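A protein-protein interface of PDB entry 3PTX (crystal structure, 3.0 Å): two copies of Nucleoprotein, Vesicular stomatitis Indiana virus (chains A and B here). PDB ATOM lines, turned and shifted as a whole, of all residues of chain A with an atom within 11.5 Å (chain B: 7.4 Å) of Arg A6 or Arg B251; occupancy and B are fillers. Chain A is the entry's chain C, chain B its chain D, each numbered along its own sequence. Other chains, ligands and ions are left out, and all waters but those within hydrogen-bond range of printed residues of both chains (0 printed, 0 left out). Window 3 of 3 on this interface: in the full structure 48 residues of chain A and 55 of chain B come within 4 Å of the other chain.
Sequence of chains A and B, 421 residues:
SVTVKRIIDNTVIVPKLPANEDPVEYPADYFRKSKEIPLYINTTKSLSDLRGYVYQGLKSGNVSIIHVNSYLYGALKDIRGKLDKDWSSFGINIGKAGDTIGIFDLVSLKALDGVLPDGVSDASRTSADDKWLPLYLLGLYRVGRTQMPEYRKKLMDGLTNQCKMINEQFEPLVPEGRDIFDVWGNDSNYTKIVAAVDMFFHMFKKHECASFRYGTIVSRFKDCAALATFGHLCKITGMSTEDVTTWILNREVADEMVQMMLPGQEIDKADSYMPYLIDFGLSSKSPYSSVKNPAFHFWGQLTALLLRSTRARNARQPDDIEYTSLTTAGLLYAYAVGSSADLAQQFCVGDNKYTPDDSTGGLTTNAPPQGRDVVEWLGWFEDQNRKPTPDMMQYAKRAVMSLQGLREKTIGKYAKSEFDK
Printed residues of chain A that touch a printed residue of chain B: Arg A6 and Ile A13.
Hydrophobic or aromatic side chains of chain A within 4 Å of the printed part of chain B: Ile A13.
Of the 14 printed residues of chain B, 5 touch a printed residue of chain A.
Hydrophobic or aromatic side chains of chain B that line the printed part of chain A: Ala B254, Met B257 and Val B258.
Among the printed residues, 6 pairs touch across the chains.
The guanidinium group (NH2) of Arg A6 sits close to the guanidinium group (NH1) of Arg B251.
The guanidinium group of Arg A6 is in salt-bridge range of the side-chain carboxylate of Asp B255 (2.6 Å).
Arg A6 touches Ala B254 (NE to CB, 3.8 Å).
CG2 of Val B258 touches NH1 of Arg A6, at 3.4 Å.
Ile A13 touches Met B257.
CA of Val B258 touches CD1 of Ile A13 (3.7 Å).
O of Val A4 is in hydrogen-bond range of N of Ile A13.
The backbone NH of Arg A6 is in hydrogen-bond range of the backbone carbonyl oxygen of Thr A11, 2.7 Å away.
The guanidinium group of Arg B251 lies within salt-bridge range of the side-chain carboxylate of Asp B255 (2.7 Å).
No position is printed for both chains.
Arg A6 touches just these residues of chain B: Arg B251, Ala B254, Asp B255 and Val B258.
Printed residues of chain B within 4 Å of Ile A13: Met B257 (3.7 Å) and Val B258 (3.7 Å).
Leu B249 touches none of the printed residues of chain A.
No residue of chain A comes within 4 Å of Asn B250.
Of chain A, only Arg A6 comes within 4 Å of Arg B251.
No residue of chain A comes within 4 Å of Glu B252.
Of chain A, only Arg A6 comes within 4 Å of Ala B254.
Of chain A, only Arg A6 comes within 4 Å of Asp B255.
Of the printed residues of chain A, Met B257 touches Ile A13 (3.7 Å).
Val B258 touches two residues of chain A.
The nearest residue of chain B that does not touch Arg A6 is Glu B252 (5.9 Å).
The nearest residue of chain A that does not touch Arg B251 is Ile A8 (4.8 Å).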
ATOM      1  N   VAL A   2     -19.187  -7.304  -9.876  1.00  0.00           N
ATOM      2  CA  VAL A   2     -19.388  -6.325  -8.802  1.00  0.00           C
ATOM      3  C   VAL A   2     -18.117  -6.290  -7.969  1.00  0.00           C
ATOM      4  O   VAL A   2     -17.804  -5.281  -7.342  1.00  0.00           O
ATOM      5  CB  VAL A   2     -20.577  -6.658  -7.834  1.00  0.00           C
ATOM      6  CG1 VAL A   2     -21.060  -5.384  -7.094  1.00  0.00           C
ATOM      7  CG2 VAL A   2     -21.733  -7.345  -8.561  1.00  0.00           C
ATOM      8  N   THR A   3     -17.382  -7.399  -7.972  1.00  0.00           N
ATOM      9  CA  THR A   3     -16.289  -7.596  -7.023  1.00  0.00           C
ATOM     10  C   THR A   3     -15.003  -8.123  -7.643  1.00  0.00           C
ATOM     11  O   THR A   3     -14.881  -9.328  -7.888  1.00  0.00           O
ATOM     12  CB  THR A   3     -16.707  -8.558  -5.900  1.00  0.00           C
ATOM     13  OG1 THR A   3     -15.561  -8.915  -5.119  1.00  0.00           O
ATOM     14  CG2 THR A   3     -17.345  -9.830  -6.482  1.00  0.00           C
ATOM     15  N   VAL A   4     -14.039  -7.218  -7.857  1.00  0.00           N
ATOM     16  CA  VAL A   4     -12.772  -7.531  -8.528  1.00  0.00           C
ATOM     17  C   VAL A   4     -11.691  -7.894  -7.526  1.00  0.00           C
ATOM     18  O   VAL A   4     -11.675  -7.367  -6.431  1.00  0.00           O
ATOM     19  CB  VAL A   4     -12.259  -6.338  -9.359  1.00  0.00           C
ATOM     20  CG1 VAL A   4     -10.915  -6.678 -10.004  1.00  0.00           C
ATOM     21  CG2 VAL A   4     -13.283  -5.902 -10.417  1.00  0.00           C
ATOM     22  N   LYS A   5     -10.796  -8.801  -7.902  1.00  0.00           N
ATOM     23  CA  LYS A   5      -9.660  -9.154  -7.062  1.00  0.00           C
ATOM     24  C   LYS A   5      -8.418  -9.357  -7.916  1.00  0.00           C
ATOM     25  O   LYS A   5      -8.516  -9.801  -9.058  1.00  0.00           O
ATOM     26  CB  LYS A   5      -9.948 -10.422  -6.258  1.00  0.00           C
ATOM     27  CG  LYS A   5      -9.984 -11.696  -7.080  1.00  0.00           C
ATOM     28  CD  LYS A   5     -10.400 -12.900  -6.231  1.00  0.00           C
ATOM     29  CE  LYS A   5     -10.584 -14.189  -7.066  1.00  0.00           C
ATOM     30  NZ  LYS A   5      -9.300 -14.741  -7.616  1.00  0.00           N
ATOM     31  N   ARG A   6      -7.256  -9.019  -7.366  1.00  0.00           N
ATOM     32  CA  ARG A   6      -5.981  -9.286  -8.023  1.00  0.00           C
ATOM     33  C   ARG A   6      -5.768 -10.789  -7.980  1.00  0.00           C
ATOM     34  O   ARG A   6      -6.099 -11.400  -6.987  1.00  0.00           O
ATOM     35  CB  ARG A   6      -4.856  -8.585  -7.253  1.00  0.00           C
ATOM     36  CG  ARG A   6      -3.453  -8.716  -7.849  1.00  0.00           C
ATOM     37  CD  ARG A   6      -3.105  -7.463  -8.572  1.00  0.00           C
ATOM     38  NE  ARG A   6      -1.697  -7.353  -8.925  1.00  0.00           N
ATOM     39  CZ  ARG A   6      -0.800  -6.702  -8.197  1.00  0.00           C
ATOM     40  NH1 ARG A   6      -1.157  -6.128  -7.045  1.00  0.00           N
ATOM     41  NH2 ARG A   6       0.457  -6.640  -8.621  1.00  0.00           N
ATOM     42  N   ILE A   7      -5.239 -11.400  -9.036  1.00  0.00           N
ATOM     43  CA  ILE A   7      -4.837 -12.800  -8.917  1.00  0.00           C
ATOM     44  C   ILE A   7      -3.648 -13.510  -8.232  1.00  0.00           C
ATOM     45  O   ILE A   7      -3.860 -14.468  -7.492  1.00  0.00           O
ATOM     46  CB  ILE A   7      -4.816 -13.549 -10.296  1.00  0.00           C
ATOM     47  CG1 ILE A   7      -3.540 -13.303 -11.099  1.00  0.00           C
ATOM     48  CG2 ILE A   7      -5.983 -13.121 -11.174  1.00  0.00           C
ATOM     49  CD1 ILE A   7      -3.642 -13.785 -12.552  1.00  0.00           C
ATOM     50  N   ILE A   8      -2.418 -13.059  -8.451  1.00  0.00           N
ATOM     51  CA  ILE A   8      -1.235 -13.646  -7.781  1.00  0.00           C
ATOM     52  C   ILE A   8      -1.263 -13.671  -6.244  1.00  0.00           C
ATOM     53  O   ILE A   8      -1.047 -14.726  -5.646  1.00  0.00           O
ATOM     54  CB  ILE A   8      -0.232 -12.551  -8.299  1.00  0.00           C
ATOM     55  CG1 ILE A   8       1.174 -12.843  -7.754  1.00  0.00           C
ATOM     56  CG2 ILE A   8      -0.696 -11.131  -7.975  1.00  0.00           C
ATOM     57  CD1 ILE A   8       1.618 -14.324  -7.959  1.00  0.00           C
ATOM     58  N   ASP A   9      -1.496 -12.525  -5.604  1.00  0.00           N
ATOM     59  CA  ASP A   9      -1.593 -12.487  -4.143  1.00  0.00           C
ATOM     60  C   ASP A   9      -3.048 -12.608  -3.673  1.00  0.00           C
ATOM     61  O   ASP A   9      -3.339 -12.791  -2.487  1.00  0.00           O
ATOM     62  CB  ASP A   9      -0.900 -11.244  -3.560  1.00  0.00           C
ATOM     63  CG  ASP A   9      -1.642  -9.955  -3.857  1.00  0.00           C
ATOM     64  OD1 ASP A   9      -0.974  -8.906  -3.997  1.00  0.00           O
ATOM     65  OD2 ASP A   9      -2.889  -9.987  -3.936  1.00  0.00           O
ATOM     66  N   ASN A  10      -3.956 -12.507  -4.630  1.00  0.00           N
ATOM     67  CA  ASN A  10      -5.380 -12.755  -4.396  1.00  0.00           C
ATOM     68  C   ASN A  10      -6.044 -11.846  -3.365  1.00  0.00           C
ATOM     69  O   ASN A  10      -6.864 -12.282  -2.560  1.00  0.00           O
ATOM     70  CB  ASN A  10      -5.648 -14.234  -4.078  1.00  0.00           C
ATOM     71  CG  ASN A  10      -6.947 -14.725  -4.684  1.00  0.00           C
ATOM     72  OD1 ASN A  10      -8.022 -14.440  -4.156  1.00  0.00           O
ATOM     73  ND2 ASN A  10      -6.858 -15.447  -5.810  1.00  0.00           N
ATOM     74  N   THR A  11      -5.689 -10.569  -3.424  1.00  0.00           N
ATOM     75  CA  THR A  11      -6.330  -9.543  -2.616  1.00  0.00           C
ATOM     76  C   THR A  11      -7.394  -8.828  -3.445  1.00  0.00           C
ATOM     77  O   THR A  11      -7.290  -8.757  -4.679  1.00  0.00           O
ATOM     78  CB  THR A  11      -5.300  -8.506  -2.093  1.00  0.00           C
ATOM     79  OG1 THR A  11      -4.618  -7.886  -3.196  1.00  0.00           O
ATOM     80  CG2 THR A  11      -4.277  -9.178  -1.176  1.00  0.00           C
ATOM     81  N   VAL A  12      -8.417  -8.303  -2.772  1.00  0.00           N
ATOM     82  CA  VAL A  12      -9.453  -7.532  -3.457  1.00  0.00           C
ATOM     83  C   VAL A  12      -8.899  -6.190  -3.887  1.00  0.00           C
ATOM     84  O   VAL A  12      -7.817  -5.775  -3.472  1.00  0.00           O
ATOM     85  CB  VAL A  12     -10.676  -7.257  -2.570  1.00  0.00           C
ATOM     86  CG1 VAL A  12     -11.847  -6.741  -3.406  1.00  0.00           C
ATOM     87  CG2 VAL A  12     -11.073  -8.500  -1.826  1.00  0.00           C
ATOM     88  N   ILE A  13      -9.649  -5.528  -4.750  1.00  0.00           N
ATOM     89  CA  ILE A  13      -9.391  -4.160  -5.127  1.00  0.00           C
ATOM     90  C   ILE A  13     -10.777  -3.642  -5.479  1.00  0.00           C
ATOM     91  O   ILE A  13     -11.580  -4.371  -6.056  1.00  0.00           O
ATOM     92  CB  ILE A  13      -8.372  -4.059  -6.322  1.00  0.00           C
ATOM     93  CG1 ILE A  13      -8.095  -2.595  -6.702  1.00  0.00           C
ATOM     94  CG2 ILE A  13      -8.849  -4.842  -7.543  1.00  0.00           C
ATOM     95  CD1 ILE A  13      -7.188  -2.425  -7.905  1.00  0.00           C
ATOM     96  N   VAL A  14     -11.098  -2.418  -5.084  1.00  0.00           N
ATOM     97  CA  VAL A  14     -12.351  -1.829  -5.537  1.00  0.00           C
ATOM     98  C   VAL A  14     -12.075  -0.729  -6.542  1.00  0.00           C
ATOM     99  O   VAL A  14     -11.783   0.400  -6.152  1.00  0.00           O
ATOM    100  CB  VAL A  14     -13.140  -1.187  -4.403  1.00  0.00           C
ATOM    101  CG1 VAL A  14     -14.506  -0.732  -4.922  1.00  0.00           C
ATOM    102  CG2 VAL A  14     -13.284  -2.140  -3.237  1.00  0.00           C
ATOM    103  N   PRO A  15     -12.136  -1.057  -7.841  1.00  0.00           N
ATOM    104  CA  PRO A  15     -12.031   0.015  -8.829  1.00  0.00           C
ATOM    105  C   PRO A  15     -13.193   0.971  -8.651  1.00  0.00           C
ATOM    106  O   PRO A  15     -14.364   0.626  -8.835  1.00  0.00           O
ATOM    107  CB  PRO A  15     -12.117  -0.722 -10.162  1.00  0.00           C
ATOM    108  CG  PRO A  15     -11.542  -2.066  -9.850  1.00  0.00           C
ATOM    109  CD  PRO A  15     -12.075  -2.384  -8.469  1.00  0.00           C
ATOM    110  N   ILE B 248      -6.278  -4.931 -17.300  1.00  0.00           N
ATOM    111  CA  ILE B 248      -4.896  -4.633 -16.952  1.00  0.00           C
ATOM    112  C   ILE B 248      -4.083  -5.918 -17.046  1.00  0.00           C
ATOM    113  O   ILE B 248      -4.399  -6.920 -16.386  1.00  0.00           O
ATOM    114  CB  ILE B 248      -4.802  -4.039 -15.547  1.00  0.00           C
ATOM    115  CG1 ILE B 248      -5.415  -2.646 -15.547  1.00  0.00           C
ATOM    116  CG2 ILE B 248      -3.372  -3.981 -15.060  1.00  0.00           C
ATOM    117  CD1 ILE B 248      -5.703  -2.133 -14.191  1.00  0.00           C
ATOM    118  N   LEU B 249      -3.045  -5.887 -17.878  1.00  0.00           N
ATOM    119  CA  LEU B 249      -2.336  -7.093 -18.265  1.00  0.00           C
ATOM    120  C   LEU B 249      -0.837  -7.037 -17.988  1.00  0.00           C
ATOM    121  O   LEU B 249      -0.068  -7.746 -18.642  1.00  0.00           O
ATOM    122  CB  LEU B 249      -2.568  -7.350 -19.745  1.00  0.00           C
ATOM    123  CG  LEU B 249      -4.007  -7.621 -20.165  1.00  0.00           C
ATOM    124  CD1 LEU B 249      -4.193  -7.555 -21.690  1.00  0.00           C
ATOM    125  CD2 LEU B 249      -4.453  -8.970 -19.611  1.00  0.00           C
ATOM    126  N   ASN B 250      -0.421  -6.196 -17.036  1.00  0.00           N
ATOM    127  CA  ASN B 250       0.992  -6.068 -16.661  1.00  0.00           C
ATOM    128  C   ASN B 250       1.149  -5.873 -15.157  1.00  0.00           C
ATOM    129  O   ASN B 250       0.487  -5.024 -14.575  1.00  0.00           O
ATOM    130  CB  ASN B 250       1.629  -4.892 -17.391  1.00  0.00           C
ATOM    131  CG  ASN B 250       1.273  -4.863 -18.855  1.00  0.00           C
ATOM    132  OD1 ASN B 250       0.156  -4.463 -19.221  1.00  0.00           O
ATOM    133  ND2 ASN B 250       2.223  -5.277 -19.714  1.00  0.00           N
ATOM    134  N   ARG B 251       2.020  -6.658 -14.525  1.00  0.00           N
ATOM    135  CA  ARG B 251       2.242  -6.519 -13.086  1.00  0.00           C
ATOM    136  C   ARG B 251       2.256  -5.051 -12.693  1.00  0.00           C
ATOM    137  O   ARG B 251       1.455  -4.618 -11.875  1.00  0.00           O
ATOM    138  CB  ARG B 251       3.541  -7.207 -12.627  1.00  0.00           C
ATOM    139  CG  ARG B 251       3.343  -8.504 -11.807  1.00  0.00           C
ATOM    140  CD  ARG B 251       2.830  -8.257 -10.370  1.00  0.00           C
ATOM    141  NE  ARG B 251       3.717  -7.379  -9.594  1.00  0.00           N
ATOM    142  CZ  ARG B 251       3.744  -7.299  -8.263  1.00  0.00           C
ATOM    143  NH1 ARG B 251       2.940  -8.058  -7.531  1.00  0.00           N
ATOM    144  NH2 ARG B 251       4.589  -6.464  -7.659  1.00  0.00           N
ATOM    145  N   GLU B 252       3.147  -4.273 -13.297  1.00  0.00           N
ATOM    146  CA  GLU B 252       3.369  -2.906 -12.838  1.00  0.00           C
ATOM    147  C   GLU B 252       2.281  -1.930 -13.255  1.00  0.00           C
ATOM    148  O   GLU B 252       2.274  -0.806 -12.795  1.00  0.00           O
ATOM    149  CB  GLU B 252       4.764  -2.386 -13.198  1.00  0.00           C
ATOM    150  CG  GLU B 252       5.211  -2.732 -14.606  1.00  0.00           C
ATOM    151  CD  GLU B 252       5.215  -4.244 -14.882  1.00  0.00           C
ATOM    152  OE1 GLU B 252       6.062  -4.970 -14.296  1.00  0.00           O
ATOM    153  OE2 GLU B 252       4.364  -4.698 -15.688  1.00  0.00           O
ATOM    154  N   VAL B 253       1.345  -2.345 -14.097  1.00  0.00           N
ATOM    155  CA  VAL B 253       0.166  -1.508 -14.321  1.00  0.00           C
ATOM    156  C   VAL B 253      -0.908  -1.816 -13.278  1.00  0.00           C
ATOM    157  O   VAL B 253      -1.656  -0.939 -12.851  1.00  0.00           O
ATOM    158  CB  VAL B 253      -0.453  -1.718 -15.700  1.00  0.00           C
ATOM    159  CG1 VAL B 253      -1.737  -0.927 -15.798  1.00  0.00           C
ATOM    160  CG2 VAL B 253       0.491  -1.295 -16.770  1.00  0.00           C
ATOM    161  N   ALA B 254      -0.987  -3.087 -12.896  1.00  0.00           N
ATOM    162  CA  ALA B 254      -1.898  -3.528 -11.860  1.00  0.00           C
ATOM    163  C   ALA B 254      -1.386  -3.052 -10.515  1.00  0.00           C
ATOM    164  O   ALA B 254      -2.162  -2.696  -9.644  1.00  0.00           O
ATOM    165  CB  ALA B 254      -2.007  -5.032 -11.876  1.00  0.00           C
ATOM    166  N   ASP B 255      -0.071  -3.049 -10.348  1.00  0.00           N
ATOM    167  CA  ASP B 255       0.509  -2.606  -9.098  1.00  0.00           C
ATOM    168  C   ASP B 255       0.060  -1.183  -8.831  1.00  0.00           C
ATOM    169  O   ASP B 255      -0.286  -0.820  -7.693  1.00  0.00           O
ATOM    170  CB  ASP B 255       2.030  -2.670  -9.151  1.00  0.00           C
ATOM    171  CG  ASP B 255       2.576  -4.002  -8.682  1.00  0.00           C
ATOM    172  OD1 ASP B 255       3.680  -4.393  -9.118  1.00  0.00           O
ATOM    173  OD2 ASP B 255       1.907  -4.660  -7.868  1.00  0.00           O
ATOM    174  N   GLU B 256       0.062  -0.386  -9.898  1.00  0.00           N
ATOM    175  CA  GLU B 256      -0.297   1.032  -9.824  1.00  0.00           C
ATOM    176  C   GLU B 256      -1.795   1.200  -9.653  1.00  0.00           C
ATOM    177  O   GLU B 256      -2.253   2.073  -8.907  1.00  0.00           O
ATOM    178  CB  GLU B 256       0.184   1.740 -11.077  1.00  0.00           C
ATOM    179  CG  GLU B 256       1.641   1.472 -11.294  1.00  0.00           C
ATOM    180  CD  GLU B 256       2.205   2.161 -12.510  1.00  0.00           C
ATOM    181  OE1 GLU B 256       3.452   2.113 -12.665  1.00  0.00           O
ATOM    182  OE2 GLU B 256       1.415   2.739 -13.299  1.00  0.00           O
ATOM    183  N   MET B 257      -2.548   0.344 -10.342  1.00  0.00           N
ATOM    184  CA  MET B 257      -3.980   0.364 -10.237  1.00  0.00           C
ATOM    185  C   MET B 257      -4.316   0.065  -8.798  1.00  0.00           C
ATOM    186  O   MET B 257      -5.219   0.667  -8.221  1.00  0.00           O
ATOM    187  CB  MET B 257      -4.591  -0.666 -11.170  1.00  0.00           C
ATOM    188  CG  MET B 257      -6.103  -0.631 -11.213  1.00  0.00           C
ATOM    189  SD  MET B 257      -6.697   1.048 -11.399  1.00  0.00           S
ATOM    190  CE  MET B 257      -8.433   0.770 -11.679  1.00  0.00           C
ATOM    191  N   VAL B 258      -3.575  -0.861  -8.207  1.00  0.00           N
ATOM    192  CA  VAL B 258      -3.828  -1.239  -6.826  1.00  0.00           C
ATOM    193  C   VAL B 258      -3.524  -0.069  -5.927  1.00  0.00           C
ATOM    194  O   VAL B 258      -4.297   0.239  -5.011  1.00  0.00           O
ATOM    195  CB  VAL B 258      -2.959  -2.409  -6.377  1.00  0.00           C
ATOM    196  CG1 VAL B 258      -2.858  -2.418  -4.869  1.00  0.00           C
ATOM    197  CG2 VAL B 258      -3.536  -3.709  -6.884  1.00  0.00           C
ATOM    198  N   GLN B 259      -2.389   0.575  -6.199  1.00  0.00           N
ATOM    199  CA  GLN B 259      -1.957   1.751  -5.456  1.00  0.00           C
ATOM    200  C   GLN B 259      -2.997   2.867  -5.543  1.00  0.00           C
ATOM    201  O   GLN B 259      -3.333   3.481  -4.541  1.00  0.00           O
ATOM    202  CB  GLN B 259      -0.588   2.192  -5.962  1.00  0.00           C
ATOM    203  CG  GLN B 259      -0.234   3.646  -5.747  1.00  0.00           C
ATOM    204  CD  GLN B 259       0.831   4.109  -6.726  1.00  0.00           C
ATOM    205  OE1 GLN B 259       1.894   3.502  -6.835  1.00  0.00           O
ATOM    206  NE2 GLN B 259       0.538   5.171  -7.464  1.00  0.00           N
ATOM    207  N   ALA B 295       3.178   3.381 -16.099  1.00  0.00           N
ATOM    208  CA  ALA B 295       2.735   2.253 -16.894  1.00  0.00           C
ATOM    209  C   ALA B 295       1.243   2.355 -17.073  1.00  0.00           C
ATOM    210  O   ALA B 295       0.725   2.195 -18.178  1.00  0.00           O
ATOM    211  CB  ALA B 295       3.099   0.954 -16.227  1.00  0.00           C
ATOM    212  N   LEU B 326       3.412  -2.885 -22.778  1.00  0.00           N
ATOM    213  CA  LEU B 326       2.335  -1.977 -22.478  1.00  0.00           C
ATOM    214  C   LEU B 326       1.580  -1.697 -23.765  1.00  0.00           C
ATOM    215  O   LEU B 326       0.357  -1.603 -23.751  1.00  0.00           O
ATOM    216  CB  LEU B 326       2.886  -0.677 -21.894  1.00  0.00           C
ATOM    217  CG  LEU B 326       2.758  -0.511 -20.374  1.00  0.00           C
ATOM    218  CD1 LEU B 326       2.192  -1.770 -19.758  1.00  0.00           C
ATOM    219  CD2 LEU B 326       4.101  -0.126 -19.729  1.00  0.00           C
